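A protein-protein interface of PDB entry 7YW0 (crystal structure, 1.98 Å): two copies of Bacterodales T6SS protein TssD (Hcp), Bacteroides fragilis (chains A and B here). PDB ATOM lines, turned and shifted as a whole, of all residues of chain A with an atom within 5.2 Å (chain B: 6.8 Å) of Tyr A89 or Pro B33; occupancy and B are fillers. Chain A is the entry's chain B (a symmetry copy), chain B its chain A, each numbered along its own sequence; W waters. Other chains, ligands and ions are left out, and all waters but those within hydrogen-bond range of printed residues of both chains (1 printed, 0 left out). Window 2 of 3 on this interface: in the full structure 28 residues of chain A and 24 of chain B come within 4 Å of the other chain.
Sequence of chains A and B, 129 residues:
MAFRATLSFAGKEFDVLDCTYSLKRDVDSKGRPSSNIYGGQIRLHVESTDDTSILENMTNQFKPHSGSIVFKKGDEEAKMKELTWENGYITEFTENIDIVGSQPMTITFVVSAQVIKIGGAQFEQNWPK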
ATOM      1  N   PHE A  62      -5.185  -2.143  23.863  1.00  0.00           N
ATOM      2  CA  PHE A  62      -3.894  -2.404  23.243  1.00  0.00           C
ATOM      3  C   PHE A  62      -4.045  -3.105  21.888  1.00  0.00           C
ATOM      4  O   PHE A  62      -3.038  -3.391  21.246  1.00  0.00           O
ATOM      5  CB  PHE A  62      -3.022  -3.223  24.204  1.00  0.00           C
ATOM      6  CG  PHE A  62      -1.617  -2.699  24.449  1.00  0.00           C
ATOM      7  CD1 PHE A  62      -1.021  -1.824  23.516  1.00  0.00           C
ATOM      8  CD2 PHE A  62      -0.896  -3.057  25.641  1.00  0.00           C
ATOM      9  CE1 PHE A  62       0.260  -1.334  23.774  1.00  0.00           C
ATOM     10  CE2 PHE A  62       0.388  -2.570  25.893  1.00  0.00           C
ATOM     11  CZ  PHE A  62       0.965  -1.709  24.956  1.00  0.00           C
ATOM     12  N   LYS A  63      -5.298  -3.373  21.470  1.00  0.00           N
ATOM     13  CA  LYS A  63      -5.624  -4.140  20.275  1.00  0.00           C
ATOM     14  C   LYS A  63      -5.714  -3.211  19.062  1.00  0.00           C
ATOM     15  O   LYS A  63      -6.318  -2.141  19.145  1.00  0.00           O
ATOM     16  CB  LYS A  63      -7.006  -4.789  20.418  1.00  0.00           C
ATOM     17  CG  LYS A  63      -7.067  -6.198  21.007  1.00  0.00           C
ATOM     18  CD  LYS A  63      -8.317  -6.960  20.573  1.00  0.00           C
ATOM     19  CE  LYS A  63      -9.214  -7.446  21.698  1.00  0.00           C
ATOM     20  NZ  LYS A  63      -8.463  -7.921  22.886  1.00  0.00           N
ATOM     21  N   PRO A  64      -5.212  -3.625  17.874  1.00  0.00           N
ATOM     22  CA  PRO A  64      -5.256  -2.774  16.677  1.00  0.00           C
ATOM     23  C   PRO A  64      -6.720  -2.520  16.319  1.00  0.00           C
ATOM     24  O   PRO A  64      -7.600  -3.258  16.772  1.00  0.00           O
ATOM     25  CB  PRO A  64      -4.545  -3.637  15.622  1.00  0.00           C
ATOM     26  CG  PRO A  64      -4.761  -5.077  16.114  1.00  0.00           C
ATOM     27  CD  PRO A  64      -4.627  -4.954  17.616  1.00  0.00           C
ATOM     28  N   HIS A  65      -6.998  -1.449  15.556  1.00  0.00           N
ATOM     29  CA  HIS A  65      -8.370  -1.194  15.120  1.00  0.00           C
ATOM     30  C   HIS A  65      -8.432  -0.749  13.659  1.00  0.00           C
ATOM     31  O   HIS A  65      -7.407  -0.552  13.005  1.00  0.00           O
ATOM     32  CB  HIS A  65      -9.038  -0.145  15.994  1.00  0.00           C
ATOM     33  CG  HIS A  65      -8.094   0.962  16.317  1.00  0.00           C
ATOM     34  ND1 HIS A  65      -7.521   1.787  15.349  1.00  0.00           N
ATOM     35  CD2 HIS A  65      -7.565   1.344  17.496  1.00  0.00           C
ATOM     36  CE1 HIS A  65      -6.736   2.671  15.929  1.00  0.00           C
ATOM     37  NE2 HIS A  65      -6.727   2.413  17.250  1.00  0.00           N
ATOM     38  N   ASN A  87      -5.787  -2.221  10.986  1.00  0.00           N
ATOM     39  CA  ASN A  87      -4.676  -2.635  11.830  1.00  0.00           C
ATOM     40  C   ASN A  87      -3.916  -1.392  12.291  1.00  0.00           C
ATOM     41  O   ASN A  87      -2.693  -1.273  12.152  1.00  0.00           O
ATOM     42  CB  ASN A  87      -3.828  -3.699  11.129  1.00  0.00           C
ATOM     43  CG  ASN A  87      -3.219  -4.729  12.056  1.00  0.00           C
ATOM     44  OD1 ASN A  87      -1.999  -4.825  12.156  1.00  0.00           O
ATOM     45  ND2 ASN A  87      -4.057  -5.528  12.706  1.00  0.00           N
ATOM     46  N   GLY A  88      -4.649  -0.445  12.878  1.00  0.00           N
ATOM     47  CA  GLY A  88      -3.956   0.756  13.322  1.00  0.00           C
ATOM     48  C   GLY A  88      -4.068   1.020  14.824  1.00  0.00           C
ATOM     49  O   GLY A  88      -4.904   0.433  15.512  1.00  0.00           O
ATOM     50  N   TYR A  89      -3.297   2.018  15.258  1.00  0.00           N
ATOM     51  CA  TYR A  89      -3.085   2.415  16.638  1.00  0.00           C
ATOM     52  C   TYR A  89      -3.035   3.933  16.695  1.00  0.00           C
ATOM     53  O   TYR A  89      -2.468   4.589  15.814  1.00  0.00           O
ATOM     54  CB  TYR A  89      -1.704   1.952  17.112  1.00  0.00           C
ATOM     55  CG  TYR A  89      -1.536   0.457  17.116  1.00  0.00           C
ATOM     56  CD1 TYR A  89      -1.979  -0.304  18.191  1.00  0.00           C
ATOM     57  CD2 TYR A  89      -0.973  -0.207  16.035  1.00  0.00           C
ATOM     58  CE1 TYR A  89      -1.879  -1.686  18.200  1.00  0.00           C
ATOM     59  CE2 TYR A  89      -0.834  -1.590  16.043  1.00  0.00           C
ATOM     60  CZ  TYR A  89      -1.293  -2.331  17.125  1.00  0.00           C
ATOM     61  OH  TYR A  89      -1.188  -3.693  17.151  1.00  0.00           O
ATOM     62  N   ILE A  90      -3.603   4.496  17.758  1.00  0.00           N
ATOM     63  CA  ILE A  90      -3.548   5.937  17.920  1.00  0.00           C
ATOM     64  C   ILE A  90      -2.213   6.268  18.568  1.00  0.00           C
ATOM     65  O   ILE A  90      -1.962   5.866  19.696  1.00  0.00           O
ATOM     66  CB  ILE A  90      -4.718   6.431  18.782  1.00  0.00           C
ATOM     67  CG1 ILE A  90      -6.074   6.328  18.087  1.00  0.00           C
ATOM     68  CG2 ILE A  90      -4.433   7.821  19.344  1.00  0.00           C
ATOM     69  CD1 ILE A  90      -7.227   6.595  19.068  1.00  0.00           C
ATOM     70  N   THR A  91      -1.381   7.039  17.872  1.00  0.00           N
ATOM     71  CA  THR A  91      -0.025   7.215  18.348  1.00  0.00           C
ATOM     72  C   THR A  91       0.217   8.659  18.767  1.00  0.00           C
ATOM     73  O   THR A  91       1.305   9.013  19.220  1.00  0.00           O
ATOM     74  CB  THR A  91       0.983   6.750  17.288  1.00  0.00           C
ATOM     75  OG1 THR A  91       0.807   7.556  16.132  1.00  0.00           O
ATOM     76  CG2 THR A  91       0.774   5.304  16.913  1.00  0.00           C
ATOM     77  N   VAL A 110      -3.551  11.159  15.757  1.00  0.00           N
ATOM     78  CA  VAL A 110      -2.886  10.566  14.608  1.00  0.00           C
ATOM     79  C   VAL A 110      -3.066   9.049  14.711  1.00  0.00           C
ATOM     80  O   VAL A 110      -2.923   8.500  15.794  1.00  0.00           O
ATOM     81  CB  VAL A 110      -1.390  10.935  14.582  1.00  0.00           C
ATOM     82  CG1 VAL A 110      -0.602  10.118  13.574  1.00  0.00           C
ATOM     83  CG2 VAL A 110      -1.146  12.421  14.378  1.00  0.00           C
ATOM     84  N   VAL A 111      -3.416   8.400  13.601  1.00  0.00           N
ATOM     85  CA  VAL A 111      -3.496   6.948  13.521  1.00  0.00           C
ATOM     86  C   VAL A 111      -2.296   6.475  12.707  1.00  0.00           C
ATOM     87  O   VAL A 111      -2.014   7.004  11.628  1.00  0.00           O
ATOM     88  CB  VAL A 111      -4.812   6.467  12.869  1.00  0.00           C
ATOM     89  CG1 VAL A 111      -4.833   4.958  12.594  1.00  0.00           C
ATOM     90  CG2 VAL A 111      -6.059   6.933  13.609  1.00  0.00           C
ATOM     91  N   SER A 112      -1.618   5.449  13.227  1.00  0.00           N
ATOM     92  CA  SER A 112      -0.585   4.762  12.479  1.00  0.00           C
ATOM     93  C   SER A 112      -1.089   3.349  12.182  1.00  0.00           C
ATOM     94  O   SER A 112      -1.363   2.587  13.105  1.00  0.00           O
ATOM     95  CB  SER A 112       0.706   4.752  13.260  1.00  0.00           C
ATOM     96  OG  SER A 112       1.771   4.493  12.359  1.00  0.00           O
ATOM     97  N   ALA A 113      -1.262   3.020  10.891  1.00  0.00           N
ATOM     98  CA  ALA A 113      -1.936   1.790  10.495  1.00  0.00           C
ATOM     99  C   ALA A 113      -1.090   1.021   9.483  1.00  0.00           C
ATOM    100  O   ALA A 113      -0.375   1.610   8.679  1.00  0.00           O
ATOM    101  CB  ALA A 113      -3.294   2.122   9.936  1.00  0.00           C
ATOM    102  N   TRP A 127       5.392  -4.971   7.654  1.00  0.00           N
ATOM    103  CA  TRP A 127       5.405  -5.368   9.051  1.00  0.00           C
ATOM    104  C   TRP A 127       5.721  -6.851   9.218  1.00  0.00           C
ATOM    105  O   TRP A 127       6.792  -7.227   9.689  1.00  0.00           O
ATOM    106  CB  TRP A 127       4.075  -5.010   9.751  1.00  0.00           C
ATOM    107  CG  TRP A 127       3.846  -3.527  10.112  1.00  0.00           C
ATOM    108  CD1 TRP A 127       4.631  -2.485   9.802  1.00  0.00           C
ATOM    109  CD2 TRP A 127       2.759  -2.990  10.848  1.00  0.00           C
ATOM    110  NE1 TRP A 127       4.121  -1.344  10.291  1.00  0.00           N
ATOM    111  CE2 TRP A 127       2.959  -1.626  10.938  1.00  0.00           C
ATOM    112  CE3 TRP A 127       1.638  -3.538  11.441  1.00  0.00           C
ATOM    113  CZ2 TRP A 127       2.080  -0.793  11.582  1.00  0.00           C
ATOM    114  CZ3 TRP A 127       0.774  -2.710  12.095  1.00  0.00           C
ATOM    115  CH2 TRP A 127       0.998  -1.357  12.156  1.00  0.00           C
ATOM    116  N   ARG B  25       2.994   8.101  21.380  1.00  0.00           N
ATOM    117  CA  ARG B  25       3.805   6.891  21.316  1.00  0.00           C
ATOM    118  C   ARG B  25       4.722   6.977  20.101  1.00  0.00           C
ATOM    119  O   ARG B  25       4.306   7.448  19.064  1.00  0.00           O
ATOM    120  CB  ARG B  25       2.912   5.679  21.031  1.00  0.00           C
ATOM    121  CG  ARG B  25       1.944   5.389  22.166  1.00  0.00           C
ATOM    122  CD  ARG B  25       0.977   4.283  21.845  1.00  0.00           C
ATOM    123  NE  ARG B  25       1.756   3.078  21.644  1.00  0.00           N
ATOM    124  CZ  ARG B  25       1.195   1.896  21.431  1.00  0.00           C
ATOM    125  NH1 ARG B  25      -0.126   1.797  21.408  1.00  0.00           N
ATOM    126  NH2 ARG B  25       1.952   0.826  21.240  1.00  0.00           N
ATOM    127  N   ASP B  26       5.950   6.476  20.207  1.00  0.00           N
ATOM    128  CA  ASP B  26       6.861   6.481  19.072  1.00  0.00           C
ATOM    129  C   ASP B  26       6.414   5.466  18.021  1.00  0.00           C
ATOM    130  O   ASP B  26       5.665   4.533  18.319  1.00  0.00           O
ATOM    131  CB  ASP B  26       8.309   6.248  19.516  1.00  0.00           C
ATOM    132  CG  ASP B  26       8.777   7.266  20.535  1.00  0.00           C
ATOM    133  OD1 ASP B  26       8.341   8.437  20.441  1.00  0.00           O
ATOM    134  OD2 ASP B  26       9.533   6.866  21.458  1.00  0.00           O
ATOM    135  N   VAL B  27       6.895   5.657  16.786  1.00  0.00           N
ATOM    136  CA  VAL B  27       6.670   4.712  15.699  1.00  0.00           C
ATOM    137  C   VAL B  27       8.002   4.443  15.003  1.00  0.00           C
ATOM    138  O   VAL B  27       8.797   5.361  14.814  1.00  0.00           O
ATOM    139  CB  VAL B  27       5.598   5.228  14.716  1.00  0.00           C
ATOM    140  N   ASP B  28       8.243   3.184  14.625  1.00  0.00           N
ATOM    141  CA  ASP B  28       9.473   2.830  13.926  1.00  0.00           C
ATOM    142  C   ASP B  28       9.383   3.239  12.448  1.00  0.00           C
ATOM    143  O   ASP B  28       8.523   4.041  12.070  1.00  0.00           O
ATOM    144  CB  ASP B  28       9.873   1.378  14.195  1.00  0.00           C
ATOM    145  CG  ASP B  28       8.795   0.401  13.777  1.00  0.00           C
ATOM    146  OD1 ASP B  28       8.231   0.610  12.691  1.00  0.00           O
ATOM    147  OD2 ASP B  28       8.496  -0.533  14.552  1.00  0.00           O
ATOM    148  N   GLY B  31       6.560   2.049  10.583  1.00  0.00           N
ATOM    149  CA  GLY B  31       5.411   2.776  11.100  1.00  0.00           C
ATOM    150  C   GLY B  31       4.674   2.025  12.217  1.00  0.00           C
ATOM    151  O   GLY B  31       3.556   2.391  12.571  1.00  0.00           O
ATOM    152  N   ARG B  32       5.287   0.964  12.756  1.00  0.00           N
ATOM    153  CA  ARG B  32       4.735   0.229  13.888  1.00  0.00           C
ATOM    154  C   ARG B  32       4.986   1.031  15.168  1.00  0.00           C
ATOM    155  O   ARG B  32       6.060   1.613  15.345  1.00  0.00           O
ATOM    156  CB  ARG B  32       5.313  -1.194  13.921  1.00  0.00           C
ATOM    157  N   PRO B  33       3.990   1.151  16.082  1.00  0.00           N
ATOM    158  CA  PRO B  33       4.218   1.790  17.385  1.00  0.00           C
ATOM    159  C   PRO B  33       5.351   1.075  18.113  1.00  0.00           C
ATOM    160  O   PRO B  33       5.388  -0.147  18.135  1.00  0.00           O
ATOM    161  CB  PRO B  33       2.887   1.656  18.139  1.00  0.00           C
ATOM    162  CG  PRO B  33       1.851   1.431  17.041  1.00  0.00           C
ATOM    163  CD  PRO B  33       2.583   0.766  15.886  1.00  0.00           C
ATOM    164  N   SER B  34       6.271   1.851  18.697  1.00  0.00           N
ATOM    165  CA  SER B  34       7.571   1.338  19.098  1.00  0.00           C
ATOM    166  C   SER B  34       7.949   1.846  20.491  1.00  0.00           C
ATOM    167  O   SER B  34       9.128   2.031  20.796  1.00  0.00           O
ATOM    168  CB  SER B  34       8.619   1.719  18.072  1.00  0.00           C
ATOM    169  OG  SER B  34       8.680   3.136  17.892  1.00  0.00           O
ATOM    170  N   SER B  35       6.930   2.065  21.329  1.00  0.00           N
ATOM    171  CA  SER B  35       7.109   2.643  22.649  1.00  0.00           C
ATOM    172  C   SER B  35       5.791   2.545  23.404  1.00  0.00           C
ATOM    173  O   SER B  35       4.730   2.376  22.808  1.00  0.00           O
ATOM    174  CB  SER B  35       7.576   4.082  22.555  1.00  0.00           C
ATOM    175  OG  SER B  35       6.585   4.979  23.037  1.00  0.00           O
HETATM  176  O   HOH W   1      -2.193   3.366  20.896  1.00  0.00           O
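The backbone carbonyl oxygen (O) of Gly B31 is in hydrogen-bond range of the side-chain hydroxyl (OG) of Ser A112 (2.8 Å). The backbone NH (N) of Arg B25 sits at hydrogen-bond distance from the backbone carbonyl oxygen (O) of Thr A91, at 2.9 Å.
No position is printed for both chains. Of the 7 pairs that touch across the chains among the printed residues, none has its exchanged pair printed and touching as well.
Phe A62 touches Arg B25 (CE1 to NH2, 3.7 Å). Pro B33 touches Tyr A89 (CG to CD2, 3.4 Å). O of Ile A90 touches CD of Arg B25 (3.97 Å). CZ2 of Trp A127 touches O of Gly B31, 3.6 Å away. Arg B32 touches Trp A127.
Water W1 bridges NH1 of Arg B25 and O of Ile A90.
The backbone NH of Ser A112 is in hydrogen-bond range of the backbone carbonyl oxygen of Tyr A89, 2.9 Å away. The guanidinium group (NE) of Arg B25 is in hydrogen-bond range of the backbone carbonyl oxygen (O) of Ser B35 (3.3 Å). The backbone NH of Gly B31 lies within hydrogen-bond range of the side-chain carboxylate of Asp B28, at 3.1 Å. The backbone NH (N) of Thr A91 lies within hydrogen-bond range of the backbone carbonyl oxygen (O) of Val A110 (3.0 Å). The side-chain carboxylate (OD1) of Asp B28 lies within hydrogen-bond range of the backbone NH (N) of Arg B32 (3.0 Å).
Of the 14 printed residues of chain A, 6 touch a printed residue of chain B. Printed residues of chain A that touch a printed residue of chain B: Phe A62, Tyr A89, Ile A90, Thr A91, Ser A112 and Trp A127. Among the printed residues, no Asp or Glu carboxylate lies within 4 Å of a Lys or Arg side-chain nitrogen of the other chain.
Tyr A89 touches just one residue of chain B: Pro B33 (3.4 Å). Of chain A, only Tyr A89 comes within 4 Å of Pro B33. Printed residues of chain B within 4 Å of Trp A127: Gly B31 and Arg B32. Of the printed residues of chain A, Arg B32 touches Trp A127 (3.6 Å). Of the printed residues of chain B, Ile A90 touches Arg B25. Printed residues of chain A within 4 Å of Arg B25: Phe A62, Ile A90 and Thr A91. Gly A88 touches none of the printed residues of chain B. The nearest residue of chain A that does not touch Pro B33 is Thr A91 (4.02 Å).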
